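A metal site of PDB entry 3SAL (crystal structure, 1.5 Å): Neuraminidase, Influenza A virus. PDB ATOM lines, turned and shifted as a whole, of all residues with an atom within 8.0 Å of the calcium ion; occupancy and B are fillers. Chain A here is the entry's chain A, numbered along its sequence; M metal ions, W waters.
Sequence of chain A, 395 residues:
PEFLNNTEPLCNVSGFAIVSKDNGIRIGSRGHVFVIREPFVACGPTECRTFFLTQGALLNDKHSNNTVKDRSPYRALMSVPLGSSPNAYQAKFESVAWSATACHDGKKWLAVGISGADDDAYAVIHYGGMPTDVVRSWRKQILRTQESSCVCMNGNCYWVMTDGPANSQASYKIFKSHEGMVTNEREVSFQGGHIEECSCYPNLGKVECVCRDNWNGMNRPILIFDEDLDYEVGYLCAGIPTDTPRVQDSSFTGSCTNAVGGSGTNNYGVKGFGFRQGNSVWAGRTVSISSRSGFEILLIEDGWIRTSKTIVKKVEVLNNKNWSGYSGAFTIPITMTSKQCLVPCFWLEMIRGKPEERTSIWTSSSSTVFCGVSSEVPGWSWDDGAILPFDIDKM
Water W1 bridges O of Pro 245 (2.7 Å) and O of Thr 265 (2.7 Å). Water W2 lies within hydrogen-bond range of the backbone carbonyl oxygen (O) of Trp 215, the backbone carbonyl oxygen (O) of Thr 265, the backbone NH (N) of Asn 267 and the backbone NH (N) of Gly 217.
CA of Gly 269 touches the calcium ion (3.9 Å). Within 4 Å of the calcium ion: Asp 213, Gly 217, Asp 243, Tyr 268 and Gly 269.
OD1 of Asp 213 lies within hydrogen-bond range of N of Gly 217 (3.0 Å). The side-chain carboxylate of Asp 213 lies within hydrogen-bond range of the backbone NH of Trp 215 (2.7 Å). The side-chain carboxylate (OD1) of Asp 213 sits at hydrogen-bond distance from the backbone NH (N) of Asn 216, 3.1 Å away. The side-chain carboxylate of Asp 213 sits at hydrogen-bond distance from the side-chain hydroxyl of Tyr 235 (2.5 Å). The backbone carbonyl oxygen (O) of Met 218 lies close to the backbone NH (N) of Asp 243 (3.2 Å). OD1 of Asp 243 is in hydrogen-bond range of N of Val 270. The side-chain amide oxygen (OD1) of Asn 214 lies within hydrogen-bond range of the backbone NH (N) of Gly 269. The guanidinium group of Arg 212 lies within hydrogen-bond range of the backbone carbonyl oxygen of Gly 269 (3.2 Å).
The calcium ion is bound by O of Asp 213 (2.4 Å), OD2 of Asp 243 (2.4 Å), O of Tyr 268 (2.4 Å), O of Gly 217 (2.5 Å), water W2 (2.5 Å) and water W1 (2.5 Å).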
ATOM      1  N   HIS A 194      20.017  13.355  -6.321  1.00  0.00           N
ATOM      2  CA  HIS A 194      20.968  12.432  -5.696  1.00  0.00           C
ATOM      3  C   HIS A 194      22.273  13.158  -5.422  1.00  0.00           C
ATOM      4  O   HIS A 194      22.817  13.823  -6.305  1.00  0.00           O
ATOM      5  CB  HIS A 194      21.207  11.229  -6.617  1.00  0.00           C
ATOM      6  CG  HIS A 194      21.769  10.038  -5.902  1.00  0.00           C
ATOM      7  ND1 HIS A 194      23.092   9.676  -6.003  1.00  0.00           N
ATOM      8  CD2 HIS A 194      21.187   9.128  -5.085  1.00  0.00           C
ATOM      9  CE1 HIS A 194      23.306   8.594  -5.271  1.00  0.00           C
ATOM     10  NE2 HIS A 194      22.167   8.248  -4.700  1.00  0.00           N
ATOM     11  N   CYS A 211      28.380  18.577  -6.328  1.00  0.00           N
ATOM     12  CA  CYS A 211      28.411  17.162  -5.966  1.00  0.00           C
ATOM     13  C   CYS A 211      28.276  16.220  -7.148  1.00  0.00           C
ATOM     14  O   CYS A 211      28.396  16.621  -8.305  1.00  0.00           O
ATOM     15  CB  CYS A 211      27.333  16.876  -4.912  1.00  0.00           C
ATOM     16  SG  CYS A 211      27.246  18.118  -3.575  1.00  0.00           S
ATOM     17  N   ARG A 212      28.048  14.941  -6.837  1.00  0.00           N
ATOM     18  CA  ARG A 212      27.897  13.903  -7.841  1.00  0.00           C
ATOM     19  C   ARG A 212      26.519  13.274  -7.696  1.00  0.00           C
ATOM     20  O   ARG A 212      26.127  12.842  -6.618  1.00  0.00           O
ATOM     21  CB  ARG A 212      28.981  12.833  -7.634  1.00  0.00           C
ATOM     22  CG  ARG A 212      28.706  11.491  -8.294  1.00  0.00           C
ATOM     23  CD  ARG A 212      29.818  10.496  -7.949  1.00  0.00           C
ATOM     24  NE  ARG A 212      29.572   9.155  -8.472  1.00  0.00           N
ATOM     25  CZ  ARG A 212      30.463   8.175  -8.445  1.00  0.00           C
ATOM     26  NH1 ARG A 212      31.659   8.393  -7.918  1.00  0.00           N
ATOM     27  NH2 ARG A 212      30.161   6.981  -8.933  1.00  0.00           N
ATOM     28  N   ASP A 213      25.769  13.262  -8.794  1.00  0.00           N
ATOM     29  CA  ASP A 213      24.487  12.566  -8.847  1.00  0.00           C
ATOM     30  C   ASP A 213      24.750  11.202  -9.442  1.00  0.00           C
ATOM     31  O   ASP A 213      25.210  11.098 -10.571  1.00  0.00           O
ATOM     32  CB  ASP A 213      23.499  13.366  -9.720  1.00  0.00           C
ATOM     33  CG  ASP A 213      22.161  12.665  -9.895  1.00  0.00           C
ATOM     34  OD1 ASP A 213      22.138  11.471 -10.235  1.00  0.00           O
ATOM     35  OD2 ASP A 213      21.123  13.337  -9.707  1.00  0.00           O
ATOM     36  N   ASN A 214      24.498  10.142  -8.678  1.00  0.00           N
ATOM     37  CA  ASN A 214      24.787   8.786  -9.130  1.00  0.00           C
ATOM     38  C   ASN A 214      23.530   8.059  -9.589  1.00  0.00           C
ATOM     39  O   ASN A 214      23.503   6.834  -9.697  1.00  0.00           O
ATOM     40  CB  ASN A 214      25.469   7.990  -8.012  1.00  0.00           C
ATOM     41  CG  ASN A 214      26.437   6.957  -8.525  1.00  0.00           C
ATOM     42  OD1 ASN A 214      27.309   7.250  -9.344  1.00  0.00           O
ATOM     43  ND2 ASN A 214      26.301   5.720  -8.043  1.00  0.00           N
ATOM     44  N   TRP A 215      22.482   8.850  -9.861  1.00  0.00           N
ATOM     45  CA  TRP A 215      21.156   8.332 -10.180  1.00  0.00           C
ATOM     46  C   TRP A 215      20.749   8.783 -11.587  1.00  0.00           C
ATOM     47  O   TRP A 215      21.205   8.207 -12.574  1.00  0.00           O
ATOM     48  CB  TRP A 215      20.166   8.813  -9.115  1.00  0.00           C
ATOM     49  CG  TRP A 215      18.777   8.261  -9.181  1.00  0.00           C
ATOM     50  CD1 TRP A 215      18.324   7.233  -9.952  1.00  0.00           C
ATOM     51  CD2 TRP A 215      17.649   8.716  -8.418  1.00  0.00           C
ATOM     52  NE1 TRP A 215      16.979   7.021  -9.725  1.00  0.00           N
ATOM     53  CE2 TRP A 215      16.541   7.915  -8.789  1.00  0.00           C
ATOM     54  CE3 TRP A 215      17.467   9.727  -7.464  1.00  0.00           C
ATOM     55  CZ2 TRP A 215      15.274   8.100  -8.235  1.00  0.00           C
ATOM     56  CZ3 TRP A 215      16.210   9.908  -6.919  1.00  0.00           C
ATOM     57  CH2 TRP A 215      15.123   9.099  -7.307  1.00  0.00           C
ATOM     58  N   ASN A 216      19.924   9.819 -11.677  1.00  0.00           N
ATOM     59  CA  ASN A 216      19.389  10.263 -12.968  1.00  0.00           C
ATOM     60  C   ASN A 216      20.068  11.488 -13.603  1.00  0.00           C
ATOM     61  O   ASN A 216      19.597  11.994 -14.617  1.00  0.00           O
ATOM     62  CB  ASN A 216      17.889  10.540 -12.852  1.00  0.00           C
ATOM     63  CG  ASN A 216      17.070   9.276 -12.666  1.00  0.00           C
ATOM     64  OD1 ASN A 216      16.088   9.261 -11.918  1.00  0.00           O
ATOM     65  ND2 ASN A 216      17.473   8.216 -13.345  1.00  0.00           N
ATOM     66  N   GLY A 217      21.147  11.981 -13.013  1.00  0.00           N
ATOM     67  CA  GLY A 217      21.732  13.224 -13.503  1.00  0.00           C
ATOM     68  C   GLY A 217      23.149  13.152 -14.014  1.00  0.00           C
ATOM     69  O   GLY A 217      24.038  12.630 -13.334  1.00  0.00           O
ATOM     70  N   MET A 218      23.376  13.683 -15.220  1.00  0.00           N
ATOM     71  CA  MET A 218      24.737  13.873 -15.740  1.00  0.00           C
ATOM     72  C   MET A 218      25.181  15.305 -15.474  1.00  0.00           C
ATOM     73  O   MET A 218      26.336  15.669 -15.735  1.00  0.00           O
ATOM     74  CB  MET A 218      24.804  13.544 -17.231  1.00  0.00           C
ATOM     75  CG  MET A 218      24.241  14.644 -18.123  1.00  0.00           C
ATOM     76  SD  MET A 218      24.307  14.224 -19.882  1.00  0.00           S
ATOM     77  CE  MET A 218      22.814  13.251 -20.064  1.00  0.00           C
ATOM     78  N   ASN A 219      24.249  16.129 -15.002  1.00  0.00           N
ATOM     79  CA  ASN A 219      24.606  17.425 -14.430  1.00  0.00           C
ATOM     80  C   ASN A 219      24.864  17.262 -12.935  1.00  0.00           C
ATOM     81  O   ASN A 219      24.405  16.309 -12.308  1.00  0.00           O
ATOM     82  CB  ASN A 219      23.545  18.498 -14.727  1.00  0.00           C
ATOM     83  CG  ASN A 219      22.119  18.075 -14.392  1.00  0.00           C
ATOM     84  OD1 ASN A 219      21.837  16.906 -14.118  1.00  0.00           O
ATOM     85  ND2 ASN A 219      21.199  19.038 -14.422  1.00  0.00           N
ATOM     86  N   ARG A 220      25.638  18.189 -12.366  1.00  0.00           N
ATOM     87  CA  ARG A 220      26.042  18.085 -10.969  1.00  0.00           C
ATOM     88  C   ARG A 220      25.096  18.818 -10.032  1.00  0.00           C
ATOM     89  O   ARG A 220      24.726  19.962 -10.299  1.00  0.00           O
ATOM     90  CB  ARG A 220      27.463  18.598 -10.777  1.00  0.00           C
ATOM     91  CG  ARG A 220      28.504  17.743 -11.462  1.00  0.00           C
ATOM     92  CD  ARG A 220      29.900  18.038 -10.930  1.00  0.00           C
ATOM     93  NE  ARG A 220      30.896  17.180 -11.551  1.00  0.00           N
ATOM     94  CZ  ARG A 220      31.111  15.911 -11.201  1.00  0.00           C
ATOM     95  NH1 ARG A 220      30.389  15.370 -10.233  1.00  0.00           N
ATOM     96  NH2 ARG A 220      32.029  15.188 -11.831  1.00  0.00           N
ATOM     97  N   PRO A 221      24.708  18.174  -8.927  1.00  0.00           N
ATOM     98  CA  PRO A 221      23.920  18.862  -7.906  1.00  0.00           C
ATOM     99  C   PRO A 221      24.706  20.013  -7.304  1.00  0.00           C
ATOM    100  O   PRO A 221      25.938  19.931  -7.176  1.00  0.00           O
ATOM    101  CB  PRO A 221      23.683  17.784  -6.850  1.00  0.00           C
ATOM    102  CG  PRO A 221      23.906  16.492  -7.550  1.00  0.00           C
ATOM    103  CD  PRO A 221      24.955  16.758  -8.583  1.00  0.00           C
ATOM    104  N   TYR A 235      20.568  21.924  -9.225  1.00  0.00           N
ATOM    105  CA  TYR A 235      21.604  21.464 -10.140  1.00  0.00           C
ATOM    106  C   TYR A 235      22.352  22.632 -10.758  1.00  0.00           C
ATOM    107  O   TYR A 235      21.814  23.728 -10.880  1.00  0.00           O
ATOM    108  CB  TYR A 235      21.010  20.562 -11.222  1.00  0.00           C
ATOM    109  CG  TYR A 235      20.687  19.191 -10.692  1.00  0.00           C
ATOM    110  CD1 TYR A 235      19.499  18.952 -10.022  1.00  0.00           C
ATOM    111  CD2 TYR A 235      21.605  18.157 -10.814  1.00  0.00           C
ATOM    112  CE1 TYR A 235      19.219  17.699  -9.510  1.00  0.00           C
ATOM    113  CE2 TYR A 235      21.330  16.900 -10.293  1.00  0.00           C
ATOM    114  CZ  TYR A 235      20.139  16.682  -9.637  1.00  0.00           C
ATOM    115  OH  TYR A 235      19.858  15.437  -9.119  1.00  0.00           O
ATOM    116  N   ASP A 243      29.503  15.909 -15.345  1.00  0.00           N
ATOM    117  CA  ASP A 243      29.720  14.593 -14.738  1.00  0.00           C
ATOM    118  C   ASP A 243      30.326  13.669 -15.794  1.00  0.00           C
ATOM    119  O   ASP A 243      30.436  14.029 -16.966  1.00  0.00           O
ATOM    120  CB  ASP A 243      28.394  14.019 -14.234  1.00  0.00           C
ATOM    121  CG  ASP A 243      28.568  12.894 -13.229  1.00  0.00           C
ATOM    122  OD1 ASP A 243      29.701  12.572 -12.828  1.00  0.00           O
ATOM    123  OD2 ASP A 243      27.535  12.338 -12.822  1.00  0.00           O
ATOM    124  N   THR A 244      30.723  12.474 -15.365  1.00  0.00           N
ATOM    125  CA  THR A 244      31.118  11.413 -16.284  1.00  0.00           C
ATOM    126  C   THR A 244      30.529  10.121 -15.740  1.00  0.00           C
ATOM    127  O   THR A 244      30.784   9.759 -14.592  1.00  0.00           O
ATOM    128  CB  THR A 244      32.638  11.266 -16.370  1.00  0.00           C
ATOM    129  OG1 THR A 244      33.224  12.531 -16.707  1.00  0.00           O
ATOM    130  CG2 THR A 244      33.022  10.224 -17.414  1.00  0.00           C
ATOM    131  N   PRO A 245      29.757   9.385 -16.560  1.00  0.00           N
ATOM    132  CA  PRO A 245      29.490   9.622 -17.985  1.00  0.00           C
ATOM    133  C   PRO A 245      28.502  10.743 -18.276  1.00  0.00           C
ATOM    134  O   PRO A 245      27.686  11.120 -17.439  1.00  0.00           O
ATOM    135  CB  PRO A 245      28.898   8.291 -18.453  1.00  0.00           C
ATOM    136  CG  PRO A 245      28.219   7.763 -17.233  1.00  0.00           C
ATOM    137  CD  PRO A 245      29.106   8.154 -16.074  1.00  0.00           C
ATOM    138  N   ARG A 246      28.593  11.278 -19.499  1.00  0.00           N
ATOM    139  CA  ARG A 246      27.689  12.321 -19.975  1.00  0.00           C
ATOM    140  C   ARG A 246      27.577  12.210 -21.485  1.00  0.00           C
ATOM    141  O   ARG A 246      28.232  11.353 -22.111  1.00  0.00           O
ATOM    142  CB  ARG A 246      28.228  13.696 -19.592  1.00  0.00           C
ATOM    143  CG  ARG A 246      29.576  14.020 -20.226  1.00  0.00           C
ATOM    144  CD  ARG A 246      30.086  15.400 -19.823  1.00  0.00           C
ATOM    145  NE  ARG A 246      31.302  15.725 -20.556  1.00  0.00           N
ATOM    146  CZ  ARG A 246      32.533  15.415 -20.159  1.00  0.00           C
ATOM    147  NH1 ARG A 246      32.722  14.784 -18.994  1.00  0.00           N
ATOM    148  NH2 ARG A 246      33.569  15.736 -20.910  1.00  0.00           N
ATOM    149  N   VAL A 260      19.290  15.911 -15.227  1.00  0.00           N
ATOM    150  CA  VAL A 260      19.195  15.654 -16.657  1.00  0.00           C
ATOM    151  C   VAL A 260      20.095  14.476 -16.973  1.00  0.00           C
ATOM    152  O   VAL A 260      21.293  14.520 -16.718  1.00  0.00           O
ATOM    153  CB  VAL A 260      19.630  16.875 -17.477  1.00  0.00           C
ATOM    154  CG1 VAL A 260      19.622  16.556 -18.969  1.00  0.00           C
ATOM    155  CG2 VAL A 260      18.733  18.062 -17.172  1.00  0.00           C
ATOM    156  N   GLY A 261      19.509  13.406 -17.502  1.00  0.00           N
ATOM    157  CA  GLY A 261      20.253  12.180 -17.706  1.00  0.00           C
ATOM    158  C   GLY A 261      19.823  11.390 -18.921  1.00  0.00           C
ATOM    159  O   GLY A 261      19.527  11.945 -19.969  1.00  0.00           O
ATOM    160  N   THR A 265      23.766   7.383 -19.461  1.00  0.00           N
ATOM    161  CA  THR A 265      24.559   8.063 -18.439  1.00  0.00           C
ATOM    162  C   THR A 265      24.060   7.809 -17.021  1.00  0.00           C
ATOM    163  O   THR A 265      24.745   8.175 -16.057  1.00  0.00           O
ATOM    164  CB  THR A 265      24.605   9.592 -18.673  1.00  0.00           C
ATOM    165  OG1 THR A 265      23.315  10.168 -18.404  1.00  0.00           O
ATOM    166  CG2 THR A 265      25.023   9.916 -20.095  1.00  0.00           C
ATOM    167  N   ASN A 266      22.892   7.204 -16.878  1.00  0.00           N
ATOM    168  CA  ASN A 266      22.306   6.982 -15.556  1.00  0.00           C
ATOM    169  C   ASN A 266      23.106   5.996 -14.702  1.00  0.00           C
ATOM    170  O   ASN A 266      23.807   5.127 -15.221  1.00  0.00           O
ATOM    171  CB  ASN A 266      20.860   6.486 -15.672  1.00  0.00           C
ATOM    172  CG  ASN A 266      19.902   7.545 -16.209  1.00  0.00           C
ATOM    173  OD1 ASN A 266      18.793   7.234 -16.621  1.00  0.00           O
ATOM    174  ND2 ASN A 266      20.333   8.800 -16.196  1.00  0.00           N
ATOM    175  N   ASN A 267      22.994   6.151 -13.389  1.00  0.00           N
ATOM    176  CA  ASN A 267      23.517   5.175 -12.420  1.00  0.00           C
ATOM    177  C   ASN A 267      25.029   5.144 -12.259  1.00  0.00           C
ATOM    178  O   ASN A 267      25.581   4.186 -11.713  1.00  0.00           O
ATOM    179  CB  ASN A 267      22.967   3.784 -12.727  1.00  0.00           C
ATOM    180  CG  ASN A 267      21.461   3.742 -12.684  1.00  0.00           C
ATOM    181  OD1 ASN A 267      20.840   4.424 -11.874  1.00  0.00           O
ATOM    182  ND2 ASN A 267      20.865   2.960 -13.560  1.00  0.00           N
ATOM    183  N   TYR A 268      25.699   6.187 -12.713  1.00  0.00           N
ATOM    184  CA  TYR A 268      27.122   6.329 -12.419  1.00  0.00           C
ATOM    185  C   TYR A 268      27.497   7.793 -12.391  1.00  0.00           C
ATOM    186  O   TYR A 268      26.637   8.658 -12.509  1.00  0.00           O
ATOM    187  CB  TYR A 268      27.979   5.559 -13.423  1.00  0.00           C
ATOM    188  CG  TYR A 268      29.324   5.115 -12.859  1.00  0.00           C
ATOM    189  CD1 TYR A 268      29.391   4.400 -11.661  1.00  0.00           C
ATOM    190  CD2 TYR A 268      30.508   5.395 -13.517  1.00  0.00           C
ATOM    191  CE1 TYR A 268      30.611   3.985 -11.145  1.00  0.00           C
ATOM    192  CE2 TYR A 268      31.734   4.980 -13.018  1.00  0.00           C
ATOM    193  CZ  TYR A 268      31.780   4.277 -11.827  1.00  0.00           C
ATOM    194  OH  TYR A 268      32.983   3.866 -11.323  1.00  0.00           O
ATOM    195  N   GLY A 269      28.780   8.066 -12.212  1.00  0.00           N
ATOM    196  CA  GLY A 269      29.261   9.423 -12.098  1.00  0.00           C
ATOM    197  C   GLY A 269      30.694   9.407 -11.636  1.00  0.00           C
ATOM    198  O   GLY A 269      31.312   8.351 -11.530  1.00  0.00           O
ATOM    199  N   VAL A 270      31.234  10.590 -11.367  1.00  0.00           N
ATOM    200  CA  VAL A 270      32.565  10.701 -10.799  1.00  0.00           C
ATOM    201  C   VAL A 270      32.566  11.924  -9.901  1.00  0.00           C
ATOM    202  O   VAL A 270      31.841  12.885 -10.158  1.00  0.00           O
ATOM    203  CB  VAL A 270      33.650  10.812 -11.898  1.00  0.00           C
ATOM    204  CG1 VAL A 270      33.511  12.122 -12.673  1.00  0.00           C
ATOM    205  CG2 VAL A 270      35.045  10.686 -11.301  1.00  0.00           C
HETATM  206 CA    CA M   1      25.673  10.853 -12.887  1.00  0.00          CA
HETATM  207  O   HOH W   1      26.155  10.414 -15.328  1.00  0.00           O
HETATM  208  O   HOH W   2      23.614   9.521 -13.341  1.00  0.00           O
